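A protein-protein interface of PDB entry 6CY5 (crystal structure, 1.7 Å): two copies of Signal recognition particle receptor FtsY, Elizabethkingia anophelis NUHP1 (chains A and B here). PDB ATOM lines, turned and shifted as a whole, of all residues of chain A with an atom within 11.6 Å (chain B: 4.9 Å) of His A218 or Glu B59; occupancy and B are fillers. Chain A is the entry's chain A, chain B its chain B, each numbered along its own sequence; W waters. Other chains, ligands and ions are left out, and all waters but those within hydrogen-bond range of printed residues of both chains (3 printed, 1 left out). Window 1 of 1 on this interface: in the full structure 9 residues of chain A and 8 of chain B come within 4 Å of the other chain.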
ATOM      1  N   GLY A 130      27.238  14.368 -14.784  1.00  0.00           N
ATOM      2  CA  GLY A 130      26.714  13.876 -13.528  1.00  0.00           C
ATOM      3  C   GLY A 130      26.065  12.521 -13.713  1.00  0.00           C
ATOM      4  O   GLY A 130      25.928  12.038 -14.843  1.00  0.00           O
ATOM      5  N   VAL A 131      25.631  11.911 -12.622  1.00  0.00           N
ATOM      6  CA  VAL A 131      25.043  10.582 -12.636  1.00  0.00           C
ATOM      7  C   VAL A 131      23.562  10.679 -12.982  1.00  0.00           C
ATOM      8  O   VAL A 131      22.911  11.690 -12.708  1.00  0.00           O
ATOM      9  CB  VAL A 131      25.282   9.918 -11.262  1.00  0.00           C
ATOM     10  CG1 VAL A 131      24.648   8.571 -11.190  1.00  0.00           C
ATOM     11  CG2 VAL A 131      26.777   9.789 -11.007  1.00  0.00           C
ATOM     12  N   ASN A 132      23.012   9.614 -13.575  1.00  0.00           N
ATOM     13  CA  ASN A 132      21.592   9.582 -13.899  1.00  0.00           C
ATOM     14  C   ASN A 132      20.738   9.858 -12.667  1.00  0.00           C
ATOM     15  O   ASN A 132      20.976   9.308 -11.587  1.00  0.00           O
ATOM     16  CB  ASN A 132      21.219   8.214 -14.479  1.00  0.00           C
ATOM     17  CG  ASN A 132      19.784   8.158 -14.969  1.00  0.00           C
ATOM     18  OD1 ASN A 132      19.488   8.587 -16.084  1.00  0.00           O
ATOM     19  ND2 ASN A 132      18.886   7.618 -14.143  1.00  0.00           N
ATOM     20  N   LYS A 136      20.259  16.490 -14.429  1.00  0.00           N
ATOM     21  CA  LYS A 136      21.036  17.093 -15.520  1.00  0.00           C
ATOM     22  C   LYS A 136      20.131  17.698 -16.583  1.00  0.00           C
ATOM     23  O   LYS A 136      20.277  18.871 -16.955  1.00  0.00           O
ATOM     24  CB  LYS A 136      21.950  16.050 -16.173  1.00  0.00           C
ATOM     25  CG  LYS A 136      23.113  15.582 -15.314  1.00  0.00           C
ATOM     26  CD  LYS A 136      23.900  14.456 -16.018  1.00  0.00           C
ATOM     27  CE  LYS A 136      23.074  13.157 -16.106  1.00  0.00           C
ATOM     28  NZ  LYS A 136      23.827  12.026 -16.765  1.00  0.00           N
ATOM     29  N   ASP A 160      23.531  12.458 -24.508  1.00  0.00           N
ATOM     30  CA  ASP A 160      23.180  11.327 -23.651  1.00  0.00           C
ATOM     31  C   ASP A 160      22.387  10.378 -24.539  1.00  0.00           C
ATOM     32  O   ASP A 160      21.198  10.593 -24.782  1.00  0.00           O
ATOM     33  CB  ASP A 160      22.373  11.799 -22.441  1.00  0.00           C
ATOM     34  CG  ASP A 160      22.095  10.687 -21.430  1.00  0.00           C
ATOM     35  OD1 ASP A 160      22.338   9.504 -21.734  1.00  0.00           O
ATOM     36  OD2 ASP A 160      21.633  11.013 -20.310  1.00  0.00           O
ATOM     37  N   PHE A 162      22.604   6.742 -24.290  1.00  0.00           N
ATOM     38  CA  PHE A 162      22.583   5.353 -23.844  1.00  0.00           C
ATOM     39  C   PHE A 162      21.161   4.807 -23.786  1.00  0.00           C
ATOM     40  O   PHE A 162      20.856   3.779 -24.402  1.00  0.00           O
ATOM     41  CB  PHE A 162      23.269   5.209 -22.488  1.00  0.00           C
ATOM     42  CG  PHE A 162      23.299   3.795 -21.992  1.00  0.00           C
ATOM     43  CD1 PHE A 162      23.862   2.791 -22.765  1.00  0.00           C
ATOM     44  CD2 PHE A 162      22.747   3.466 -20.766  1.00  0.00           C
ATOM     45  CE1 PHE A 162      23.884   1.479 -22.320  1.00  0.00           C
ATOM     46  CE2 PHE A 162      22.765   2.156 -20.313  1.00  0.00           C
ATOM     47  CZ  PHE A 162      23.332   1.161 -21.091  1.00  0.00           C
ATOM     48  N   ARG A 163      20.246   5.530 -23.148  1.00  0.00           N
ATOM     49  CA  ARG A 163      18.829   5.181 -23.184  1.00  0.00           C
ATOM     50  C   ARG A 163      18.103   6.007 -24.243  1.00  0.00           C
ATOM     51  O   ARG A 163      18.413   7.184 -24.446  1.00  0.00           O
ATOM     52  CB  ARG A 163      18.181   5.392 -21.815  1.00  0.00           C
ATOM     53  N   ALA A 214      25.593  11.263 -20.627  1.00  0.00           N
ATOM     54  CA  ALA A 214      25.411  10.189 -19.680  1.00  0.00           C
ATOM     55  C   ALA A 214      26.541  10.260 -18.665  1.00  0.00           C
ATOM     56  O   ALA A 214      27.626  10.778 -18.948  1.00  0.00           O
ATOM     57  CB  ALA A 214      25.402   8.823 -20.376  1.00  0.00           C
ATOM     58  N   GLY A 215      26.283   9.742 -17.482  1.00  0.00           N
ATOM     59  CA  GLY A 215      27.338   9.777 -16.494  1.00  0.00           C
ATOM     60  C   GLY A 215      27.324   8.514 -15.682  1.00  0.00           C
ATOM     61  O   GLY A 215      27.149   8.545 -14.462  1.00  0.00           O
ATOM     62  N   ARG A 216      27.504   7.388 -16.360  1.00  0.00           N
ATOM     63  CA  ARG A 216      27.458   6.086 -15.707  1.00  0.00           C
ATOM     64  C   ARG A 216      28.764   5.918 -14.952  1.00  0.00           C
ATOM     65  O   ARG A 216      29.800   5.597 -15.533  1.00  0.00           O
ATOM     66  CB  ARG A 216      27.242   4.984 -16.734  1.00  0.00           C
ATOM     67  CG  ARG A 216      26.056   5.253 -17.644  1.00  0.00           C
ATOM     68  CD  ARG A 216      25.991   4.213 -18.736  1.00  0.00           C
ATOM     69  NE  ARG A 216      25.571   2.915 -18.222  1.00  0.00           N
ATOM     70  CZ  ARG A 216      25.880   1.760 -18.802  1.00  0.00           C
ATOM     71  NH1 ARG A 216      26.629   1.751 -19.903  1.00  0.00           N
ATOM     72  NH2 ARG A 216      25.454   0.620 -18.286  1.00  0.00           N
ATOM     73  N   LEU A 217      28.716   6.174 -13.654  1.00  0.00           N
ATOM     74  CA  LEU A 217      29.915   6.271 -12.836  1.00  0.00           C
ATOM     75  C   LEU A 217      30.445   4.916 -12.391  1.00  0.00           C
ATOM     76  O   LEU A 217      31.564   4.850 -11.854  1.00  0.00           O
ATOM     77  CB  LEU A 217      29.593   7.158 -11.634  1.00  0.00           C
ATOM     78  CG  LEU A 217      30.651   7.670 -10.663  1.00  0.00           C
ATOM     79  CD1 LEU A 217      31.720   8.445 -11.380  1.00  0.00           C
ATOM     80  CD2 LEU A 217      29.940   8.552  -9.645  1.00  0.00           C
ATOM     81  N   HIS A 218      29.701   3.831 -12.648  1.00  0.00           N
ATOM     82  CA  HIS A 218      30.114   2.520 -12.165  1.00  0.00           C
ATOM     83  C   HIS A 218      31.411   2.052 -12.810  1.00  0.00           C
ATOM     84  O   HIS A 218      32.143   1.262 -12.203  1.00  0.00           O
ATOM     85  CB  HIS A 218      29.014   1.481 -12.402  1.00  0.00           C
ATOM     86  CG  HIS A 218      28.809   1.154 -13.844  1.00  0.00           C
ATOM     87  ND1 HIS A 218      28.091   1.970 -14.694  1.00  0.00           N
ATOM     88  CD2 HIS A 218      29.257   0.123 -14.600  1.00  0.00           C
ATOM     89  CE1 HIS A 218      28.101   1.450 -15.910  1.00  0.00           C
ATOM     90  NE2 HIS A 218      28.798   0.330 -15.880  1.00  0.00           N
ATOM     91  N   ASN A 219      31.702   2.478 -14.043  1.00  0.00           N
ATOM     92  CA  ASN A 219      32.997   2.173 -14.652  1.00  0.00           C
ATOM     93  C   ASN A 219      33.637   3.512 -14.979  1.00  0.00           C
ATOM     94  O   ASN A 219      33.327   4.131 -16.001  1.00  0.00           O
ATOM     95  CB  ASN A 219      32.875   1.284 -15.888  1.00  0.00           C
ATOM     96  CG  ASN A 219      34.245   0.857 -16.436  1.00  0.00           C
ATOM     97  OD1 ASN A 219      35.194   1.632 -16.408  1.00  0.00           O
ATOM     98  ND2 ASN A 219      34.346  -0.377 -16.928  1.00  0.00           N
ATOM     99  N   LYS A 220      34.522   3.959 -14.096  1.00  0.00           N
ATOM    100  CA  LYS A 220      35.134   5.267 -14.265  1.00  0.00           C
ATOM    101  C   LYS A 220      36.062   5.327 -15.468  1.00  0.00           C
ATOM    102  O   LYS A 220      36.295   6.416 -15.995  1.00  0.00           O
ATOM    103  CB  LYS A 220      35.896   5.646 -13.002  1.00  0.00           C
ATOM    104  CG  LYS A 220      34.972   6.062 -11.869  1.00  0.00           C
ATOM    105  CD  LYS A 220      35.761   6.340 -10.620  1.00  0.00           C
ATOM    106  CE  LYS A 220      34.855   6.563  -9.430  1.00  0.00           C
ATOM    107  NZ  LYS A 220      35.666   6.844  -8.211  1.00  0.00           N
ATOM    108  N   VAL A 221      36.593   4.193 -15.915  1.00  0.00           N
ATOM    109  CA  VAL A 221      37.401   4.217 -17.127  1.00  0.00           C
ATOM    110  C   VAL A 221      36.535   4.570 -18.328  1.00  0.00           C
ATOM    111  O   VAL A 221      36.867   5.465 -19.116  1.00  0.00           O
ATOM    112  CB  VAL A 221      38.130   2.877 -17.320  1.00  0.00           C
ATOM    113  CG1 VAL A 221      38.793   2.824 -18.697  1.00  0.00           C
ATOM    114  CG2 VAL A 221      39.178   2.703 -16.234  1.00  0.00           C
ATOM    115  N   ASN A 222      35.399   3.885 -18.485  1.00  0.00           N
ATOM    116  CA  ASN A 222      34.530   4.186 -19.620  1.00  0.00           C
ATOM    117  C   ASN A 222      34.005   5.612 -19.549  1.00  0.00           C
ATOM    118  O   ASN A 222      33.896   6.295 -20.575  1.00  0.00           O
ATOM    119  CB  ASN A 222      33.370   3.193 -19.672  1.00  0.00           C
ATOM    120  CG  ASN A 222      33.828   1.784 -19.992  1.00  0.00           C
ATOM    121  OD1 ASN A 222      34.939   1.576 -20.484  1.00  0.00           O
ATOM    122  ND2 ASN A 222      32.969   0.806 -19.725  1.00  0.00           N
ATOM    123  N   LEU A 223      33.649   6.062 -18.347  1.00  0.00           N
ATOM    124  CA  LEU A 223      33.184   7.430 -18.144  1.00  0.00           C
ATOM    125  C   LEU A 223      34.236   8.442 -18.563  1.00  0.00           C
ATOM    126  O   LEU A 223      33.952   9.382 -19.315  1.00  0.00           O
ATOM    127  CB  LEU A 223      32.833   7.635 -16.674  1.00  0.00           C
ATOM    128  CG  LEU A 223      32.440   9.073 -16.352  1.00  0.00           C
ATOM    129  CD1 LEU A 223      31.165   9.396 -17.093  1.00  0.00           C
ATOM    130  CD2 LEU A 223      32.258   9.257 -14.846  1.00  0.00           C
ATOM    131  N   MET A 224      35.456   8.269 -18.055  1.00  0.00           N
ATOM    132  CA  MET A 224      36.564   9.157 -18.375  1.00  0.00           C
ATOM    133  C   MET A 224      36.799   9.208 -19.881  1.00  0.00           C
ATOM    134  O   MET A 224      36.964  10.289 -20.460  1.00  0.00           O
ATOM    135  CB  MET A 224      37.796   8.655 -17.612  1.00  0.00           C
ATOM    136  CG  MET A 224      39.069   9.436 -17.652  1.00  0.00           C
ATOM    137  SD  MET A 224      40.021   8.923 -16.176  1.00  0.00           S
ATOM    138  CE  MET A 224      40.005   7.142 -16.312  1.00  0.00           C
ATOM    139  N   ASN A 225      36.806   8.043 -20.537  1.00  0.00           N
ATOM    140  CA  ASN A 225      37.062   7.992 -21.977  1.00  0.00           C
ATOM    141  C   ASN A 225      35.958   8.678 -22.779  1.00  0.00           C
ATOM    142  O   ASN A 225      36.238   9.355 -23.779  1.00  0.00           O
ATOM    143  CB  ASN A 225      37.218   6.540 -22.426  1.00  0.00           C
ATOM    144  CG  ASN A 225      38.506   5.913 -21.931  1.00  0.00           C
ATOM    145  OD1 ASN A 225      39.464   6.615 -21.621  1.00  0.00           O
ATOM    146  ND2 ASN A 225      38.544   4.582 -21.885  1.00  0.00           N
ATOM    147  N   GLU A 226      34.698   8.488 -22.382  1.00  0.00           N
ATOM    148  CA  GLU A 226      33.599   9.080 -23.134  1.00  0.00           C
ATOM    149  C   GLU A 226      33.636  10.596 -23.028  1.00  0.00           C
ATOM    150  O   GLU A 226      33.548  11.301 -24.036  1.00  0.00           O
ATOM    151  CB  GLU A 226      32.254   8.548 -22.634  1.00  0.00           C
ATOM    152  CG  GLU A 226      31.056   9.246 -23.295  1.00  0.00           C
ATOM    153  CD  GLU A 226      29.753   8.480 -23.139  1.00  0.00           C
ATOM    154  OE1 GLU A 226      29.766   7.238 -23.226  1.00  0.00           O
ATOM    155  OE2 GLU A 226      28.713   9.130 -22.948  1.00  0.00           O
ATOM    156  N   LEU A 227      33.774  11.115 -21.807  1.00  0.00           N
ATOM    157  CA  LEU A 227      33.808  12.559 -21.631  1.00  0.00           C
ATOM    158  C   LEU A 227      35.029  13.170 -22.310  1.00  0.00           C
ATOM    159  O   LEU A 227      34.942  14.262 -22.884  1.00  0.00           O
ATOM    160  CB  LEU A 227      33.779  12.912 -20.143  1.00  0.00           C
ATOM    161  CG  LEU A 227      32.477  12.508 -19.439  1.00  0.00           C
ATOM    162  CD1 LEU A 227      32.536  12.870 -17.974  1.00  0.00           C
ATOM    163  CD2 LEU A 227      31.248  13.157 -20.119  1.00  0.00           C
ATOM    164  N   GLN A 260      29.712  11.771  -3.910  1.00  0.00           N
ATOM    165  CA  GLN A 260      29.609  11.553  -5.348  1.00  0.00           C
ATOM    166  C   GLN A 260      30.413  12.590  -6.126  1.00  0.00           C
ATOM    167  O   GLN A 260      31.069  12.256  -7.118  1.00  0.00           O
ATOM    168  CB  GLN A 260      28.149  11.577  -5.780  1.00  0.00           C
ATOM    169  CG  GLN A 260      27.931  11.176  -7.218  1.00  0.00           C
ATOM    170  CD  GLN A 260      26.465  11.246  -7.564  1.00  0.00           C
ATOM    171  OE1 GLN A 260      25.965  12.290  -7.961  1.00  0.00           O
ATOM    172  NE2 GLN A 260      25.758  10.143  -7.351  1.00  0.00           N
ATOM    173  N   GLN A 263      33.992  11.592  -6.103  1.00  0.00           N
ATOM    174  CA  GLN A 263      34.270  10.517  -7.052  1.00  0.00           C
ATOM    175  C   GLN A 263      34.271  11.035  -8.485  1.00  0.00           C
ATOM    176  O   GLN A 263      35.162  10.695  -9.280  1.00  0.00           O
ATOM    177  CB  GLN A 263      33.241   9.392  -6.890  1.00  0.00           C
ATOM    178  CG  GLN A 263      33.165   8.795  -5.479  1.00  0.00           C
ATOM    179  CD  GLN A 263      34.412   8.022  -5.089  1.00  0.00           C
ATOM    180  OE1 GLN A 263      35.157   7.549  -5.945  1.00  0.00           O
ATOM    181  NE2 GLN A 263      34.643   7.891  -3.786  1.00  0.00           N
ATOM    182  N   PHE A 264      33.294  11.870  -8.831  1.00  0.00           N
ATOM    183  CA  PHE A 264      33.162  12.323 -10.212  1.00  0.00           C
ATOM    184  C   PHE A 264      34.292  13.278 -10.599  1.00  0.00           C
ATOM    185  O   PHE A 264      34.870  13.153 -11.684  1.00  0.00           O
ATOM    186  CB  PHE A 264      31.792  12.982 -10.417  1.00  0.00           C
ATOM    187  CG  PHE A 264      31.241  12.826 -11.820  1.00  0.00           C
ATOM    188  CD1 PHE A 264      31.764  13.555 -12.872  1.00  0.00           C
ATOM    189  CD2 PHE A 264      30.188  11.957 -12.075  1.00  0.00           C
ATOM    190  CE1 PHE A 264      31.246  13.416 -14.156  1.00  0.00           C
ATOM    191  CE2 PHE A 264      29.675  11.814 -13.356  1.00  0.00           C
ATOM    192  CZ  PHE A 264      30.210  12.539 -14.398  1.00  0.00           C
ATOM    193  N   ALA A 267      37.407  11.741 -11.704  1.00  0.00           N
ATOM    194  CA  ALA A 267      37.388  11.075 -12.999  1.00  0.00           C
ATOM    195  C   ALA A 267      37.456  12.032 -14.184  1.00  0.00           C
ATOM    196  O   ALA A 267      37.875  11.616 -15.269  1.00  0.00           O
ATOM    197  CB  ALA A 267      36.126  10.214 -13.139  1.00  0.00           C
ATOM    198  N   LEU B  55      27.758  -7.565 -19.269  1.00  0.00           N
ATOM    199  CA  LEU B  55      28.523  -7.535 -18.023  1.00  0.00           C
ATOM    200  C   LEU B  55      28.693  -6.113 -17.501  1.00  0.00           C
ATOM    201  O   LEU B  55      28.684  -5.892 -16.281  1.00  0.00           O
ATOM    202  CB  LEU B  55      29.882  -8.204 -18.222  1.00  0.00           C
ATOM    203  CG  LEU B  55      29.780  -9.684 -18.570  1.00  0.00           C
ATOM    204  CD1 LEU B  55      31.155 -10.255 -18.832  1.00  0.00           C
ATOM    205  CD2 LEU B  55      29.085 -10.415 -17.440  1.00  0.00           C
ATOM    206  N   ASP B  56      28.861  -5.140 -18.402  1.00  0.00           N
ATOM    207  CA  ASP B  56      28.906  -3.741 -17.983  1.00  0.00           C
ATOM    208  C   ASP B  56      27.593  -3.329 -17.331  1.00  0.00           C
ATOM    209  O   ASP B  56      27.578  -2.707 -16.260  1.00  0.00           O
ATOM    210  CB  ASP B  56      29.224  -2.846 -19.188  1.00  0.00           C
ATOM    211  CG  ASP B  56      29.270  -1.380 -18.827  1.00  0.00           C
ATOM    212  OD1 ASP B  56      30.004  -1.022 -17.891  1.00  0.00           O
ATOM    213  OD2 ASP B  56      28.589  -0.581 -19.507  1.00  0.00           O
ATOM    214  N   ASP B  57      26.469  -3.682 -17.958  1.00  0.00           N
ATOM    215  CA  ASP B  57      25.183  -3.341 -17.365  1.00  0.00           C
ATOM    216  C   ASP B  57      24.967  -4.077 -16.050  1.00  0.00           C
ATOM    217  O   ASP B  57      24.345  -3.532 -15.132  1.00  0.00           O
ATOM    218  CB  ASP B  57      24.061  -3.644 -18.354  1.00  0.00           C
ATOM    219  CG  ASP B  57      24.125  -2.760 -19.598  1.00  0.00           C
ATOM    220  OD1 ASP B  57      24.902  -1.775 -19.609  1.00  0.00           O
ATOM    221  OD2 ASP B  57      23.420  -3.062 -20.583  1.00  0.00           O
ATOM    222  N   LEU B  58      25.495  -5.297 -15.932  1.00  0.00           N
ATOM    223  CA  LEU B  58      25.353  -6.037 -14.686  1.00  0.00           C
ATOM    224  C   LEU B  58      26.168  -5.386 -13.579  1.00  0.00           C
ATOM    225  O   LEU B  58      25.732  -5.351 -12.424  1.00  0.00           O
ATOM    226  CB  LEU B  58      25.765  -7.494 -14.889  1.00  0.00           C
ATOM    227  CG  LEU B  58      25.690  -8.353 -13.624  1.00  0.00           C
ATOM    228  CD1 LEU B  58      24.251  -8.470 -13.102  1.00  0.00           C
ATOM    229  CD2 LEU B  58      26.304  -9.723 -13.898  1.00  0.00           C
ATOM    230  N   GLU B  59      27.346  -4.837 -13.911  1.00  0.00           N
ATOM    231  CA  GLU B  59      28.095  -4.095 -12.901  1.00  0.00           C
ATOM    232  C   GLU B  59      27.279  -2.923 -12.385  1.00  0.00           C
ATOM    233  O   GLU B  59      27.201  -2.699 -11.173  1.00  0.00           O
ATOM    234  CB  GLU B  59      29.437  -3.602 -13.453  1.00  0.00           C
ATOM    235  CG  GLU B  59      30.202  -2.773 -12.398  1.00  0.00           C
ATOM    236  CD  GLU B  59      31.615  -2.435 -12.802  1.00  0.00           C
ATOM    237  OE1 GLU B  59      32.416  -2.123 -11.892  1.00  0.00           O
ATOM    238  OE2 GLU B  59      31.923  -2.487 -14.014  1.00  0.00           O
ATOM    239  N   GLU B  60      26.636  -2.181 -13.289  1.00  0.00           N
ATOM    240  CA  GLU B  60      25.781  -1.071 -12.874  1.00  0.00           C
ATOM    241  C   GLU B  60      24.653  -1.544 -11.961  1.00  0.00           C
ATOM    242  O   GLU B  60      24.312  -0.866 -10.986  1.00  0.00           O
ATOM    243  CB  GLU B  60      25.223  -0.363 -14.108  1.00  0.00           C
ATOM    244  CG  GLU B  60      24.279   0.815 -13.859  1.00  0.00           C
ATOM    245  CD  GLU B  60      23.963   1.527 -15.169  1.00  0.00           C
ATOM    246  OE1 GLU B  60      23.570   0.836 -16.130  1.00  0.00           O
ATOM    247  OE2 GLU B  60      24.151   2.760 -15.267  1.00  0.00           O
ATOM    248  N   VAL B  61      24.060  -2.702 -12.262  1.00  0.00           N
ATOM    249  CA  VAL B  61      22.994  -3.229 -11.406  1.00  0.00           C
ATOM    250  C   VAL B  61      23.527  -3.582 -10.020  1.00  0.00           C
ATOM    251  O   VAL B  61      22.862  -3.339  -9.004  1.00  0.00           O
ATOM    252  CB  VAL B  61      22.330  -4.448 -12.069  1.00  0.00           C
ATOM    253  CG1 VAL B  61      21.482  -5.180 -11.056  1.00  0.00           C
ATOM    254  CG2 VAL B  61      21.496  -4.010 -13.292  1.00  0.00           C
ATOM    255  N   LEU B  62      24.708  -4.209  -9.952  1.00  0.00           N
ATOM    256  CA  LEU B  62      25.238  -4.602  -8.648  1.00  0.00           C
ATOM    257  C   LEU B  62      25.536  -3.381  -7.792  1.00  0.00           C
ATOM    258  O   LEU B  62      25.217  -3.361  -6.596  1.00  0.00           O
ATOM    259  CB  LEU B  62      26.488  -5.463  -8.823  1.00  0.00           C
ATOM    260  CG  LEU B  62      26.165  -6.890  -9.262  1.00  0.00           C
ATOM    261  CD1 LEU B  62      27.379  -7.569  -9.861  1.00  0.00           C
ATOM    262  CD2 LEU B  62      25.646  -7.679  -8.062  1.00  0.00           C
ATOM    263  N   ILE B  63      26.099  -2.330  -8.402  1.00  0.00           N
ATOM    264  CA  ILE B  63      26.319  -1.076  -7.680  1.00  0.00           C
ATOM    265  C   ILE B  63      24.989  -0.474  -7.224  1.00  0.00           C
ATOM    266  O   ILE B  63      24.864   0.011  -6.087  1.00  0.00           O
ATOM    267  CB  ILE B  63      27.124  -0.093  -8.557  1.00  0.00           C
ATOM    268  CG1 ILE B  63      28.534  -0.625  -8.849  1.00  0.00           C
ATOM    269  CG2 ILE B  63      27.161   1.306  -7.931  1.00  0.00           C
ATOM    270  CD1 ILE B  63      29.425  -0.814  -7.606  1.00  0.00           C
ATOM    271  N   THR B  72      31.867  -5.728  -6.148  1.00  0.00           N
ATOM    272  CA  THR B  72      31.300  -5.863  -7.483  1.00  0.00           C
ATOM    273  C   THR B  72      32.384  -6.133  -8.515  1.00  0.00           C
ATOM    274  O   THR B  72      32.189  -6.948  -9.425  1.00  0.00           O
ATOM    275  CB  THR B  72      30.500  -4.613  -7.829  1.00  0.00           C
ATOM    276  OG1 THR B  72      29.380  -4.532  -6.934  1.00  0.00           O
ATOM    277  CG2 THR B  72      30.002  -4.656  -9.300  1.00  0.00           C
ATOM    278  N   VAL B  73      33.540  -5.475  -8.385  1.00  0.00           N
ATOM    279  CA  VAL B  73      34.637  -5.741  -9.315  1.00  0.00           C
ATOM    280  C   VAL B  73      35.035  -7.212  -9.264  1.00  0.00           C
ATOM    281  O   VAL B  73      35.251  -7.846 -10.301  1.00  0.00           O
ATOM    282  CB  VAL B  73      35.838  -4.823  -9.023  1.00  0.00           C
ATOM    283  CG1 VAL B  73      37.092  -5.380  -9.670  1.00  0.00           C
ATOM    284  CG2 VAL B  73      35.570  -3.425  -9.547  1.00  0.00           C
ATOM    285  N   ILE B  76      32.264  -9.344 -11.017  1.00  0.00           N
ATOM    286  CA  ILE B  76      32.272  -9.213 -12.468  1.00  0.00           C
ATOM    287  C   ILE B  76      33.522  -9.856 -13.049  1.00  0.00           C
ATOM    288  O   ILE B  76      33.485 -10.449 -14.135  1.00  0.00           O
ATOM    289  CB  ILE B  76      32.155  -7.735 -12.874  1.00  0.00           C
ATOM    290  CG1 ILE B  76      30.792  -7.184 -12.461  1.00  0.00           C
ATOM    291  CG2 ILE B  76      32.366  -7.575 -14.387  1.00  0.00           C
ATOM    292  CD1 ILE B  76      29.640  -7.846 -13.196  1.00  0.00           C
HETATM  293  O   HOH W   1      26.267   3.781 -13.685  1.00  0.00           O
HETATM  294  O   HOH W   2      32.028  -2.232 -16.696  1.00  0.00           O
HETATM  295  O   HOH W   3      30.287   1.677 -18.992  1.00  0.00           O
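The side-chain carboxylate (OE1) of Glu B59 lies close to the backbone carbonyl oxygen (O) of His A218. The side-chain carboxylate (OD2) of Asp B56 is in salt-bridge range of the guanidinium group (NH1) of Arg A216 (3.1 Å). The side-chain carboxylate (OE1) of Glu B60 lies within salt-bridge range of the guanidinium group (NH2) of Arg A216 (2.9 Å). NH2 of Arg A216 lies within salt-bridge range of OD1 of Asp B57. The side-chain carboxylate of Asp B56 is in hydrogen-bond range of a ring nitrogen (NE2) of His A218 (2.7 Å).
The backbone NH (N) of Asn A222 sits at hydrogen-bond distance from the side-chain amide oxygen (OD1) of Asn A219 (3.1 Å).
Among the printed residues, merely in contact across the chains: Phe A162 with Asp B57, His A218 with Glu B60 and Asn A222 with Asp B56.
Arg A163 touches none of the printed residues of chain B. Printed residues of chain B within 4 Å of Arg A216: Asp B56 (3.1 Å), Asp B57 (2.8 Å) and Glu B60 (2.9 Å). Of chain B, only Asp B56 (2.7 Å), Glu B59 (3.4 Å) and Glu B60 (3.7 Å) come within 4 Å of His A218. Printed residues of chain B within 4 Å of Asn A222: Asp B56. Leu A223 touches none of the printed residues of chain B. Of chain A, only Arg A216, His A218 and Asn A222 come within 4 Å of Asp B56. Printed residues of chain A within 4 Å of Asp B57: Phe A162 and Arg A216. No residue of chain A comes within 4 Å of Leu B58. Glu B59 touches just one residue of chain A: His A218 (3.4 Å). Of chain A, only Arg A216 and His A218 come within 4 Å of Glu B60. No residue of chain A comes within 4 Å of Leu B62. Ile B63 touches none of the printed residues of chain A.
Of the 25 printed residues of chain A, 4 touch a printed residue of chain B. Hydrophobic or aromatic side chains of chain A within 4 Å of the printed part of chain B: Phe A162 and His A218. Of the 12 printed residues of chain B, 4 touch a printed residue of chain A. Printed residues of chain B that touch a printed residue of chain A: Asp B56, Asp B57, Glu B59 and Glu B60. Among the printed residues, 8 pairs touch across the chains.
No position is printed for both chains. Of the 8 pairs that touch across the chains among the printed residues, none has its exchanged pair printed and touching as well.
Water W2 lies within hydrogen-bond range of OD1 of Asp B56 (2.6 Å), OE2 of Glu B59 (2.7 Å) and ND2 of Asn A219 (3.0 Å). Water W1 lies within hydrogen-bond range of a ring nitrogen (ND1) of His A218 (2.8 Å), the side-chain carboxylate of Glu B60 (2.8 Å) and the backbone NH of Leu A217 (3.4 Å). Water W3 bridges OD2 of Asp B56 (2.9 Å) and ND2 of Asn A222 (2.9 Å).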
